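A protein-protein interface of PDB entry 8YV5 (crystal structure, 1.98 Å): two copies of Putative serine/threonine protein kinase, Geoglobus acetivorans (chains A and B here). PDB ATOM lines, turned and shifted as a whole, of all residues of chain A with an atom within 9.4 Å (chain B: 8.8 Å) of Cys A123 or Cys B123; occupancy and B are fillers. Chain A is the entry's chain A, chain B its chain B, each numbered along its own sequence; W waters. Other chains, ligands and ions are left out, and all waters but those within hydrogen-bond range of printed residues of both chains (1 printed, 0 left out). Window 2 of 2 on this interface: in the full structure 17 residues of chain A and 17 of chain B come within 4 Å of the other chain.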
ATOM      1  N   ARG A  86     -16.870   2.328   3.596  1.00  0.00           N
ATOM      2  CA  ARG A  86     -18.011   2.365   4.498  1.00  0.00           C
ATOM      3  C   ARG A  86     -17.640   1.759   5.845  1.00  0.00           C
ATOM      4  O   ARG A  86     -18.004   2.302   6.895  1.00  0.00           O
ATOM      5  CB  ARG A  86     -19.182   1.637   3.841  1.00  0.00           C
ATOM      6  CG  ARG A  86     -20.389   1.511   4.701  1.00  0.00           C
ATOM      7  CD  ARG A  86     -20.887   2.833   5.235  1.00  0.00           C
ATOM      8  NE  ARG A  86     -22.056   2.538   6.053  1.00  0.00           N
ATOM      9  CZ  ARG A  86     -22.569   3.351   6.960  1.00  0.00           C
ATOM     10  NH1 ARG A  86     -22.065   4.555   7.174  1.00  0.00           N
ATOM     11  NH2 ARG A  86     -23.579   2.921   7.711  1.00  0.00           N
ATOM     12  N   LEU A  88     -14.663   1.836   7.251  1.00  0.00           N
ATOM     13  CA  LEU A  88     -13.875   2.847   7.954  1.00  0.00           C
ATOM     14  C   LEU A  88     -14.777   3.967   8.481  1.00  0.00           C
ATOM     15  O   LEU A  88     -14.573   4.470   9.598  1.00  0.00           O
ATOM     16  CB  LEU A  88     -12.796   3.386   7.015  1.00  0.00           C
ATOM     17  CG  LEU A  88     -11.650   2.399   6.685  1.00  0.00           C
ATOM     18  CD1 LEU A  88     -10.768   2.957   5.560  1.00  0.00           C
ATOM     19  CD2 LEU A  88     -10.822   2.068   7.897  1.00  0.00           C
ATOM     20  N   ASP A  89     -15.781   4.363   7.692  1.00  0.00           N
ATOM     21  CA  ASP A  89     -16.764   5.340   8.161  1.00  0.00           C
ATOM     22  C   ASP A  89     -17.449   4.849   9.431  1.00  0.00           C
ATOM     23  O   ASP A  89     -17.607   5.598  10.404  1.00  0.00           O
ATOM     24  CB  ASP A  89     -17.812   5.587   7.083  1.00  0.00           C
ATOM     25  CG  ASP A  89     -17.310   6.461   5.945  1.00  0.00           C
ATOM     26  OD1 ASP A  89     -16.141   6.911   5.948  1.00  0.00           O
ATOM     27  OD2 ASP A  89     -18.121   6.718   5.038  1.00  0.00           O
ATOM     28  N   VAL A  90     -17.906   3.594   9.416  1.00  0.00           N
ATOM     29  CA  VAL A  90     -18.642   3.048  10.553  1.00  0.00           C
ATOM     30  C   VAL A  90     -17.751   2.967  11.786  1.00  0.00           C
ATOM     31  O   VAL A  90     -18.180   3.254  12.918  1.00  0.00           O
ATOM     32  CB  VAL A  90     -19.232   1.674  10.171  1.00  0.00           C
ATOM     33  CG1 VAL A  90     -19.876   1.023  11.372  1.00  0.00           C
ATOM     34  CG2 VAL A  90     -20.313   1.829   9.089  1.00  0.00           C
ATOM     35  N   LEU A  91     -16.481   2.624  11.582  1.00  0.00           N
ATOM     36  CA  LEU A  91     -15.501   2.463  12.653  1.00  0.00           C
ATOM     37  C   LEU A  91     -15.091   3.786  13.275  1.00  0.00           C
ATOM     38  O   LEU A  91     -14.575   3.801  14.401  1.00  0.00           O
ATOM     39  CB  LEU A  91     -14.259   1.781  12.063  1.00  0.00           C
ATOM     40  CG  LEU A  91     -14.495   0.308  11.717  1.00  0.00           C
ATOM     41  CD1 LEU A  91     -13.243  -0.332  11.104  1.00  0.00           C
ATOM     42  CD2 LEU A  91     -14.932  -0.437  12.960  1.00  0.00           C
ATOM     43  N   GLY A  92     -15.293   4.890  12.572  1.00  0.00           N
ATOM     44  CA  GLY A  92     -14.890   6.197  13.063  1.00  0.00           C
ATOM     45  C   GLY A  92     -13.511   6.631  12.635  1.00  0.00           C
ATOM     46  O   GLY A  92     -12.996   7.608  13.172  1.00  0.00           O
ATOM     47  N   ILE A  93     -12.917   5.976  11.642  1.00  0.00           N
ATOM     48  CA  ILE A  93     -11.545   6.269  11.228  1.00  0.00           C
ATOM     49  C   ILE A  93     -11.589   7.042   9.914  1.00  0.00           C
ATOM     50  O   ILE A  93     -12.010   6.519   8.870  1.00  0.00           O
ATOM     51  CB  ILE A  93     -10.716   4.985  11.127  1.00  0.00           C
ATOM     52  CG1 ILE A  93     -10.582   4.354  12.527  1.00  0.00           C
ATOM     53  CG2 ILE A  93      -9.368   5.239  10.458  1.00  0.00           C
ATOM     54  CD1 ILE A  93     -10.175   2.875  12.506  1.00  0.00           C
ATOM     55  N   GLN A  94     -11.178   8.308   9.976  1.00  0.00           N
ATOM     56  CA  GLN A  94     -11.058   9.150   8.787  1.00  0.00           C
ATOM     57  C   GLN A  94      -9.621   9.017   8.306  1.00  0.00           C
ATOM     58  O   GLN A  94      -8.699   9.588   8.888  1.00  0.00           O
ATOM     59  CB  GLN A  94     -11.454  10.593   9.086  1.00  0.00           C
ATOM     60  CG  GLN A  94     -11.078  11.604   7.988  1.00  0.00           C
ATOM     61  CD  GLN A  94     -12.147  12.661   7.718  1.00  0.00           C
ATOM     62  OE1 GLN A  94     -13.351  12.416   7.845  1.00  0.00           O
ATOM     63  NE2 GLN A  94     -11.702  13.858   7.369  1.00  0.00           N
ATOM     64  N   VAL A 120      -7.312  10.281  11.487  1.00  0.00           N
ATOM     65  CA  VAL A 120      -7.888  10.916  12.672  1.00  0.00           C
ATOM     66  C   VAL A 120      -9.210  10.217  12.970  1.00  0.00           C
ATOM     67  O   VAL A 120      -9.872   9.686  12.074  1.00  0.00           O
ATOM     68  CB  VAL A 120      -8.110  12.443  12.509  1.00  0.00           C
ATOM     69  CG1 VAL A 120      -6.815  13.155  12.197  1.00  0.00           C
ATOM     70  CG2 VAL A 120      -9.089  12.716  11.360  1.00  0.00           C
ATOM     71  N   ILE A 121      -9.595  10.231  14.240  1.00  0.00           N
ATOM     72  CA  ILE A 121     -10.909   9.672  14.644  1.00  0.00           C
ATOM     73  C   ILE A 121     -11.944  10.781  14.446  1.00  0.00           C
ATOM     74  O   ILE A 121     -11.652  11.918  14.823  1.00  0.00           O
ATOM     75  CB  ILE A 121     -10.876   9.166  16.095  1.00  0.00           C
ATOM     76  CG1 ILE A 121      -9.881   8.020  16.278  1.00  0.00           C
ATOM     77  CG2 ILE A 121     -12.267   8.785  16.570  1.00  0.00           C
ATOM     78  CD1 ILE A 121      -9.740   7.565  17.708  1.00  0.00           C
ATOM     79  N   LYS A 122     -13.070  10.455  13.822  1.00  0.00           N
ATOM     80  CA  LYS A 122     -14.123  11.455  13.527  1.00  0.00           C
ATOM     81  C   LYS A 122     -15.477  10.765  13.655  1.00  0.00           C
ATOM     82  O   LYS A 122     -15.545   9.562  13.404  1.00  0.00           O
ATOM     83  CB  LYS A 122     -13.931  12.066  12.140  1.00  0.00           C
ATOM     84  CG  LYS A 122     -13.123  13.355  12.103  1.00  0.00           C
ATOM     85  CD  LYS A 122     -13.350  14.168  10.852  1.00  0.00           C
ATOM     86  CE  LYS A 122     -14.808  14.245  10.451  1.00  0.00           C
ATOM     87  NZ  LYS A 122     -15.377  15.589  10.705  1.00  0.00           N
ATOM     88  N   CYS A 123     -16.496  11.515  14.074  1.00  0.00           N
ATOM     89  CA  CYS A 123     -17.845  10.933  14.281  1.00  0.00           C
ATOM     90  C   CYS A 123     -18.404  10.501  12.925  1.00  0.00           C
ATOM     91  O   CYS A 123     -19.024   9.436  12.859  1.00  0.00           O
ATOM     92  CB  CYS A 123     -18.781  11.958  14.911  1.00  0.00           C
ATOM     93  SG  CYS A 123     -18.347  12.407  16.611  1.00  0.00           S
ATOM     94  N   ARG A 124     -18.163  11.310  11.894  1.00  0.00           N
ATOM     95  CA  ARG A 124     -18.701  10.998  10.575  1.00  0.00           C
ATOM     96  C   ARG A 124     -17.544  11.163   9.594  1.00  0.00           C
ATOM     97  O   ARG A 124     -17.364  12.231   8.988  1.00  0.00           O
ATOM     98  CB  ARG A 124     -19.893  11.906  10.255  1.00  0.00           C
ATOM     99  N   PRO A 125     -16.718  10.127   9.434  1.00  0.00           N
ATOM    100  CA  PRO A 125     -15.582  10.223   8.509  1.00  0.00           C
ATOM    101  C   PRO A 125     -16.038  10.443   7.072  1.00  0.00           C
ATOM    102  O   PRO A 125     -17.198  10.220   6.712  1.00  0.00           O
ATOM    103  CB  PRO A 125     -14.879   8.863   8.667  1.00  0.00           C
ATOM    104  CG  PRO A 125     -15.337   8.372  10.032  1.00  0.00           C
ATOM    105  CD  PRO A 125     -16.770   8.815  10.097  1.00  0.00           C
ATOM    106  N   SER A 126     -15.079  10.868   6.245  1.00  0.00           N
ATOM    107  CA  SER A 126     -15.286  11.184   4.845  1.00  0.00           C
ATOM    108  C   SER A 126     -14.588  10.196   3.902  1.00  0.00           C
ATOM    109  O   SER A 126     -14.226  10.579   2.794  1.00  0.00           O
ATOM    110  CB  SER A 126     -14.788  12.600   4.577  1.00  0.00           C
ATOM    111  OG  SER A 126     -15.701  13.560   5.076  1.00  0.00           O
ATOM    112  N   ASN A 127     -14.416   8.927   4.301  1.00  0.00           N
ATOM    113  CA  ASN A 127     -13.745   7.961   3.422  1.00  0.00           C
ATOM    114  C   ASN A 127     -14.547   7.703   2.149  1.00  0.00           C
ATOM    115  O   ASN A 127     -13.984   7.720   1.048  1.00  0.00           O
ATOM    116  CB  ASN A 127     -13.489   6.648   4.154  1.00  0.00           C
ATOM    117  CG  ASN A 127     -12.653   6.839   5.399  1.00  0.00           C
ATOM    118  OD1 ASN A 127     -11.502   7.304   5.344  1.00  0.00           O
ATOM    119  ND2 ASN A 127     -13.256   6.557   6.538  1.00  0.00           N
ATOM    120  N   TYR A 154     -26.203  10.517   1.528  1.00  0.00           N
ATOM    121  CA  TYR A 154     -25.497   9.594   2.420  1.00  0.00           C
ATOM    122  C   TYR A 154     -25.032  10.300   3.689  1.00  0.00           C
ATOM    123  O   TYR A 154     -25.194   9.778   4.800  1.00  0.00           O
ATOM    124  CB  TYR A 154     -24.300   8.950   1.700  1.00  0.00           C
ATOM    125  CG  TYR A 154     -23.318   8.192   2.607  1.00  0.00           C
ATOM    126  CD1 TYR A 154     -23.657   6.970   3.189  1.00  0.00           C
ATOM    127  CD2 TYR A 154     -22.068   8.723   2.907  1.00  0.00           C
ATOM    128  CE1 TYR A 154     -22.771   6.286   4.002  1.00  0.00           C
ATOM    129  CE2 TYR A 154     -21.175   8.054   3.741  1.00  0.00           C
ATOM    130  CZ  TYR A 154     -21.529   6.831   4.287  1.00  0.00           C
ATOM    131  OH  TYR A 154     -20.643   6.153   5.116  1.00  0.00           O
ATOM    132  N   LYS A 155     -24.445  11.495   3.548  1.00  0.00           N
ATOM    133  CA  LYS A 155     -23.871  12.148   4.720  1.00  0.00           C
ATOM    134  C   LYS A 155     -24.945  12.532   5.728  1.00  0.00           C
ATOM    135  O   LYS A 155     -24.680  12.530   6.935  1.00  0.00           O
ATOM    136  CB  LYS A 155     -23.053  13.373   4.307  1.00  0.00           C
ATOM    137  N   PHE A 158     -26.218   8.632   6.891  1.00  0.00           N
ATOM    138  CA  PHE A 158     -25.056   7.913   7.488  1.00  0.00           C
ATOM    139  C   PHE A 158     -25.534   6.658   8.201  1.00  0.00           C
ATOM    140  O   PHE A 158     -25.249   6.498   9.390  1.00  0.00           O
ATOM    141  CB  PHE A 158     -24.237   8.815   8.411  1.00  0.00           C
ATOM    142  CG  PHE A 158     -22.745   8.625   8.321  1.00  0.00           C
ATOM    143  CD1 PHE A 158     -21.997   9.324   7.387  1.00  0.00           C
ATOM    144  CD2 PHE A 158     -22.084   7.758   9.173  1.00  0.00           C
ATOM    145  CE1 PHE A 158     -20.625   9.156   7.308  1.00  0.00           C
ATOM    146  CE2 PHE A 158     -20.712   7.590   9.093  1.00  0.00           C
ATOM    147  CZ  PHE A 158     -19.985   8.290   8.161  1.00  0.00           C
ATOM    148  N   ARG B  86     -12.411  13.462  30.167  1.00  0.00           N
ATOM    149  CA  ARG B  86     -12.950  14.362  29.147  1.00  0.00           C
ATOM    150  C   ARG B  86     -12.079  14.353  27.896  1.00  0.00           C
ATOM    151  O   ARG B  86     -12.593  14.398  26.772  1.00  0.00           O
ATOM    152  CB  ARG B  86     -13.058  15.778  29.694  1.00  0.00           C
ATOM    153  CG  ARG B  86     -13.335  16.841  28.633  1.00  0.00           C
ATOM    154  CD  ARG B  86     -14.707  16.669  27.985  1.00  0.00           C
ATOM    155  NE  ARG B  86     -14.956  17.684  26.959  1.00  0.00           N
ATOM    156  CZ  ARG B  86     -15.956  17.644  26.084  1.00  0.00           C
ATOM    157  NH1 ARG B  86     -16.852  16.652  26.090  1.00  0.00           N
ATOM    158  NH2 ARG B  86     -16.070  18.625  25.187  1.00  0.00           N
ATOM    159  N   LEU B  88     -10.268  11.907  26.720  1.00  0.00           N
ATOM    160  CA  LEU B  88     -10.607  10.692  25.979  1.00  0.00           C
ATOM    161  C   LEU B  88     -11.961  10.841  25.297  1.00  0.00           C
ATOM    162  O   LEU B  88     -12.130  10.440  24.133  1.00  0.00           O
ATOM    163  CB  LEU B  88     -10.601   9.491  26.926  1.00  0.00           C
ATOM    164  CG  LEU B  88      -9.245   9.025  27.454  1.00  0.00           C
ATOM    165  CD1 LEU B  88      -9.460   7.978  28.527  1.00  0.00           C
ATOM    166  CD2 LEU B  88      -8.344   8.414  26.342  1.00  0.00           C
ATOM    167  N   ASP B  89     -12.934  11.449  25.990  1.00  0.00           N
ATOM    168  CA  ASP B  89     -14.236  11.687  25.371  1.00  0.00           C
ATOM    169  C   ASP B  89     -14.082  12.498  24.096  1.00  0.00           C
ATOM    170  O   ASP B  89     -14.649  12.153  23.054  1.00  0.00           O
ATOM    171  CB  ASP B  89     -15.189  12.430  26.324  1.00  0.00           C
ATOM    172  CG  ASP B  89     -15.765  11.531  27.426  1.00  0.00           C
ATOM    173  OD1 ASP B  89     -15.513  10.298  27.429  1.00  0.00           O
ATOM    174  OD2 ASP B  89     -16.508  12.077  28.284  1.00  0.00           O
ATOM    175  N   VAL B  90     -13.327  13.595  24.166  1.00  0.00           N
ATOM    176  CA  VAL B  90     -13.205  14.488  23.017  1.00  0.00           C
ATOM    177  C   VAL B  90     -12.467  13.764  21.886  1.00  0.00           C
ATOM    178  O   VAL B  90     -12.788  13.950  20.709  1.00  0.00           O
ATOM    179  CB  VAL B  90     -12.496  15.796  23.424  1.00  0.00           C
ATOM    180  CG1 VAL B  90     -11.767  16.454  22.255  1.00  0.00           C
ATOM    181  CG2 VAL B  90     -13.442  16.747  24.144  1.00  0.00           C
ATOM    182  N   LEU B  91     -11.493  12.912  22.226  1.00  0.00           N
ATOM    183  CA  LEU B  91     -10.731  12.168  21.213  1.00  0.00           C
ATOM    184  C   LEU B  91     -11.557  11.072  20.545  1.00  0.00           C
ATOM    185  O   LEU B  91     -11.162  10.582  19.471  1.00  0.00           O
ATOM    186  CB  LEU B  91      -9.504  11.508  21.836  1.00  0.00           C
ATOM    187  CG  LEU B  91      -8.417  12.472  22.311  1.00  0.00           C
ATOM    188  CD1 LEU B  91      -7.372  11.698  23.070  1.00  0.00           C
ATOM    189  CD2 LEU B  91      -7.795  13.190  21.169  1.00  0.00           C
ATOM    190  N   GLY B  92     -12.649  10.635  21.172  1.00  0.00           N
ATOM    191  CA  GLY B  92     -13.476   9.578  20.604  1.00  0.00           C
ATOM    192  C   GLY B  92     -13.132   8.177  21.055  1.00  0.00           C
ATOM    193  O   GLY B  92     -13.544   7.218  20.393  1.00  0.00           O
ATOM    194  N   ILE B  93     -12.382   8.017  22.148  1.00  0.00           N
ATOM    195  CA  ILE B  93     -11.942   6.701  22.620  1.00  0.00           C
ATOM    196  C   ILE B  93     -12.730   6.344  23.868  1.00  0.00           C
ATOM    197  O   ILE B  93     -12.607   7.012  24.907  1.00  0.00           O
ATOM    198  CB  ILE B  93     -10.426   6.652  22.854  1.00  0.00           C
ATOM    199  CG1 ILE B  93      -9.729   6.858  21.502  1.00  0.00           C
ATOM    200  CG2 ILE B  93      -9.997   5.322  23.550  1.00  0.00           C
ATOM    201  CD1 ILE B  93      -8.278   7.333  21.593  1.00  0.00           C
ATOM    202  N   GLN B  94     -13.563   5.305  23.756  1.00  0.00           N
ATOM    203  CA  GLN B  94     -14.302   4.757  24.892  1.00  0.00           C
ATOM    204  C   GLN B  94     -13.458   3.655  25.500  1.00  0.00           C
ATOM    205  O   GLN B  94     -13.348   2.566  24.934  1.00  0.00           O
ATOM    206  CB  GLN B  94     -15.654   4.211  24.468  1.00  0.00           C
ATOM    207  CG  GLN B  94     -16.435   3.623  25.621  1.00  0.00           C
ATOM    208  CD  GLN B  94     -17.935   3.818  25.430  1.00  0.00           C
ATOM    209  OE1 GLN B  94     -18.399   4.944  25.239  1.00  0.00           O
ATOM    210  NE2 GLN B  94     -18.690   2.715  25.422  1.00  0.00           N
ATOM    211  N   VAL B 120     -13.033   1.045  22.510  1.00  0.00           N
ATOM    212  CA  VAL B 120     -13.805   1.091  21.240  1.00  0.00           C
ATOM    213  C   VAL B 120     -13.887   2.560  20.832  1.00  0.00           C
ATOM    214  O   VAL B 120     -13.883   3.412  21.722  1.00  0.00           O
ATOM    215  CB  VAL B 120     -15.217   0.500  21.401  1.00  0.00           C
ATOM    216  CG1 VAL B 120     -15.197  -1.010  21.564  1.00  0.00           C
ATOM    217  CG2 VAL B 120     -15.988   1.155  22.533  1.00  0.00           C
ATOM    218  N   ILE B 121     -13.931   2.843  19.538  1.00  0.00           N
ATOM    219  CA  ILE B 121     -14.120   4.247  19.089  1.00  0.00           C
ATOM    220  C   ILE B 121     -15.613   4.568  19.173  1.00  0.00           C
ATOM    221  O   ILE B 121     -16.414   3.701  18.818  1.00  0.00           O
ATOM    222  CB  ILE B 121     -13.544   4.464  17.680  1.00  0.00           C
ATOM    223  CG1 ILE B 121     -12.019   4.327  17.675  1.00  0.00           C
ATOM    224  CG2 ILE B 121     -13.990   5.796  17.103  1.00  0.00           C
ATOM    225  CD1 ILE B 121     -11.401   4.388  16.302  1.00  0.00           C
ATOM    226  N   LYS B 122     -15.952   5.756  19.672  1.00  0.00           N
ATOM    227  CA  LYS B 122     -17.367   6.179  19.783  1.00  0.00           C
ATOM    228  C   LYS B 122     -17.457   7.688  19.542  1.00  0.00           C
ATOM    229  O   LYS B 122     -16.495   8.394  19.864  1.00  0.00           O
ATOM    230  CB  LYS B 122     -17.942   5.779  21.142  1.00  0.00           C
ATOM    231  CG  LYS B 122     -18.076   4.288  21.411  1.00  0.00           C
ATOM    232  CD  LYS B 122     -19.507   3.818  21.430  1.00  0.00           C
ATOM    233  CE  LYS B 122     -19.684   2.461  20.789  1.00  0.00           C
ATOM    234  NZ  LYS B 122     -20.794   1.701  21.412  1.00  0.00           N
ATOM    235  N   CYS B 123     -18.565   8.151  18.964  1.00  0.00           N
ATOM    236  CA  CYS B 123     -18.768   9.601  18.715  1.00  0.00           C
ATOM    237  C   CYS B 123     -18.831  10.328  20.060  1.00  0.00           C
ATOM    238  O   CYS B 123     -18.236  11.398  20.170  1.00  0.00           O
ATOM    239  CB  CYS B 123     -20.074   9.867  17.972  1.00  0.00           C
ATOM    240  SG  CYS B 123     -20.103   9.268  16.262  1.00  0.00           S
ATOM    241  N   ARG B 124     -19.542   9.749  21.025  1.00  0.00           N
ATOM    242  CA  ARG B 124     -19.666  10.350  22.353  1.00  0.00           C
ATOM    243  C   ARG B 124     -19.354   9.284  23.398  1.00  0.00           C
ATOM    244  O   ARG B 124     -20.256   8.585  23.883  1.00  0.00           O
ATOM    245  CB  ARG B 124     -21.046  10.963  22.554  1.00  0.00           C
ATOM    246  CG  ARG B 124     -21.313  12.093  21.571  1.00  0.00           C
ATOM    247  CD  ARG B 124     -22.633  12.791  21.845  1.00  0.00           C
ATOM    248  NE  ARG B 124     -22.696  14.082  21.165  1.00  0.00           N
ATOM    249  CZ  ARG B 124     -23.631  15.003  21.374  1.00  0.00           C
ATOM    250  NH1 ARG B 124     -24.617  14.803  22.232  1.00  0.00           N
ATOM    251  NH2 ARG B 124     -23.570  16.155  20.708  1.00  0.00           N
ATOM    252  N   PRO B 125     -18.077   9.110  23.736  1.00  0.00           N
ATOM    253  CA  PRO B 125     -17.680   8.065  24.690  1.00  0.00           C
ATOM    254  C   PRO B 125     -18.272   8.274  26.078  1.00  0.00           C
ATOM    255  O   PRO B 125     -18.770   9.344  26.438  1.00  0.00           O
ATOM    256  CB  PRO B 125     -16.153   8.186  24.733  1.00  0.00           C
ATOM    257  CG  PRO B 125     -15.781   8.814  23.391  1.00  0.00           C
ATOM    258  CD  PRO B 125     -16.918   9.747  23.078  1.00  0.00           C
ATOM    259  N   SER B 126     -18.188   7.208  26.882  1.00  0.00           N
ATOM    260  CA  SER B 126     -18.709   7.199  28.244  1.00  0.00           C
ATOM    261  C   SER B 126     -17.608   7.146  29.310  1.00  0.00           C
ATOM    262  O   SER B 126     -17.803   6.577  30.383  1.00  0.00           O
ATOM    263  CB  SER B 126     -19.679   6.028  28.392  1.00  0.00           C
ATOM    264  OG  SER B 126     -20.760   6.219  27.488  1.00  0.00           O
ATOM    265  N   TYR B 154     -24.844  16.295  30.267  1.00  0.00           N
ATOM    266  CA  TYR B 154     -23.519  16.286  29.653  1.00  0.00           C
ATOM    267  C   TYR B 154     -23.551  15.597  28.296  1.00  0.00           C
ATOM    268  O   TYR B 154     -22.982  16.095  27.319  1.00  0.00           O
ATOM    269  CB  TYR B 154     -22.518  15.592  30.576  1.00  0.00           C
ATOM    270  CG  TYR B 154     -21.184  15.353  29.923  1.00  0.00           C
ATOM    271  CD1 TYR B 154     -20.403  16.426  29.484  1.00  0.00           C
ATOM    272  CD2 TYR B 154     -20.712  14.059  29.717  1.00  0.00           C
ATOM    273  CE1 TYR B 154     -19.165  16.208  28.871  1.00  0.00           C
ATOM    274  CE2 TYR B 154     -19.474  13.827  29.110  1.00  0.00           C
ATOM    275  CZ  TYR B 154     -18.718  14.901  28.681  1.00  0.00           C
ATOM    276  OH  TYR B 154     -17.516  14.680  28.056  1.00  0.00           O
ATOM    277  N   LYS B 155     -24.197  14.429  28.216  1.00  0.00           N
ATOM    278  CA  LYS B 155     -24.208  13.702  26.945  1.00  0.00           C
ATOM    279  C   LYS B 155     -24.984  14.468  25.882  1.00  0.00           C
ATOM    280  O   LYS B 155     -24.630  14.406  24.699  1.00  0.00           O
ATOM    281  CB  LYS B 155     -24.796  12.303  27.127  1.00  0.00           C
ATOM    282  CG  LYS B 155     -23.795  11.316  27.740  1.00  0.00           C
ATOM    283  CD  LYS B 155     -22.602  11.032  26.802  1.00  0.00           C
ATOM    284  CE  LYS B 155     -22.408   9.537  26.533  1.00  0.00           C
ATOM    285  NZ  LYS B 155     -22.443   8.690  27.782  1.00  0.00           N
ATOM    286  N   PHE B 158     -22.222  18.002  25.407  1.00  0.00           N
ATOM    287  CA  PHE B 158     -20.947  17.363  25.060  1.00  0.00           C
ATOM    288  C   PHE B 158     -19.891  18.325  24.513  1.00  0.00           C
ATOM    289  O   PHE B 158     -18.861  17.876  23.991  1.00  0.00           O
ATOM    290  CB  PHE B 158     -21.154  16.198  24.071  1.00  0.00           C
ATOM    291  CG  PHE B 158     -20.211  15.016  24.305  1.00  0.00           C
ATOM    292  CD1 PHE B 158     -20.325  14.217  25.447  1.00  0.00           C
ATOM    293  CD2 PHE B 158     -19.219  14.701  23.376  1.00  0.00           C
ATOM    294  CE1 PHE B 158     -19.476  13.138  25.666  1.00  0.00           C
ATOM    295  CE2 PHE B 158     -18.342  13.589  23.580  1.00  0.00           C
ATOM    296  CZ  PHE B 158     -18.476  12.817  24.725  1.00  0.00           C
HETATM  297  O   HOH W   1     -11.497  12.434  17.585  1.00  0.00           O
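O of Cys A123 lies close to SG of Cys B123, 3.6 Å away.
The backbone carbonyl oxygen (O) of Leu A88 lies within hydrogen-bond range of the backbone NH (N) of Ile A93, 3.0 Å away.
N of Ile B93 sits at hydrogen-bond distance from O of Leu B88 (3.1 Å).
ND2 of Asn A127 sits at hydrogen-bond distance from O of Ile A93 (2.6 Å).
Water W1 bridges O of Leu B91 (2.7 Å) and O of Ile A121 (2.8 Å).
Of the printed residues of chain B, Leu A91 touches Ile B121 (3.4 Å).
Of the printed residues of chain B, Ile A121 touches Leu B91, Ile B93 and Ile B121.
Of chain B, only Cys B123 comes within 4 Å of Cys A123.
No residue of chain B comes within 4 Å of Arg A124.
Printed residues of chain A within 4 Å of Leu B91: Ile A121.
Printed residues of chain A within 4 Å of Ile B93: Ile A121 (3.9 Å).
Printed residues of chain A within 4 Å of Ile B121: Leu A91, Ile A93 and Ile A121.
Cys B123 touches one residue of chain A.
Arg B124 touches none of the printed residues of chain A.
Of the 19 printed residues of chain A, 4 touch a printed residue of chain B.
Hydrophobic or aromatic side chains of chain A within 4 Å of the printed part of chain B: Ile A93 and Ile A121.
Leu A91 touches Ile B121 (O to CG2, 3.4 Å).
CD1 of Ile B121 touches CG1 of Ile A93, at 3.9 Å.
CG2 of Ile A121 touches O of Leu B91, 3.6 Å away.
CD1 of Ile A121 touches CG1 of Ile B93, at 3.9 Å.
Ile B121 touches Ile A121.
Leu A91 touches Ile B121, and with the chains exchanged Ile A121 touches Leu B91.
Ile A93 touches Ile B121, and with the chains exchanged Ile A121 touches Ile B93.
Ile A121 touches its own counterpart, Ile B121.
Cys B123 touches its own counterpart, Cys A123.
18 positions are printed for both chains.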
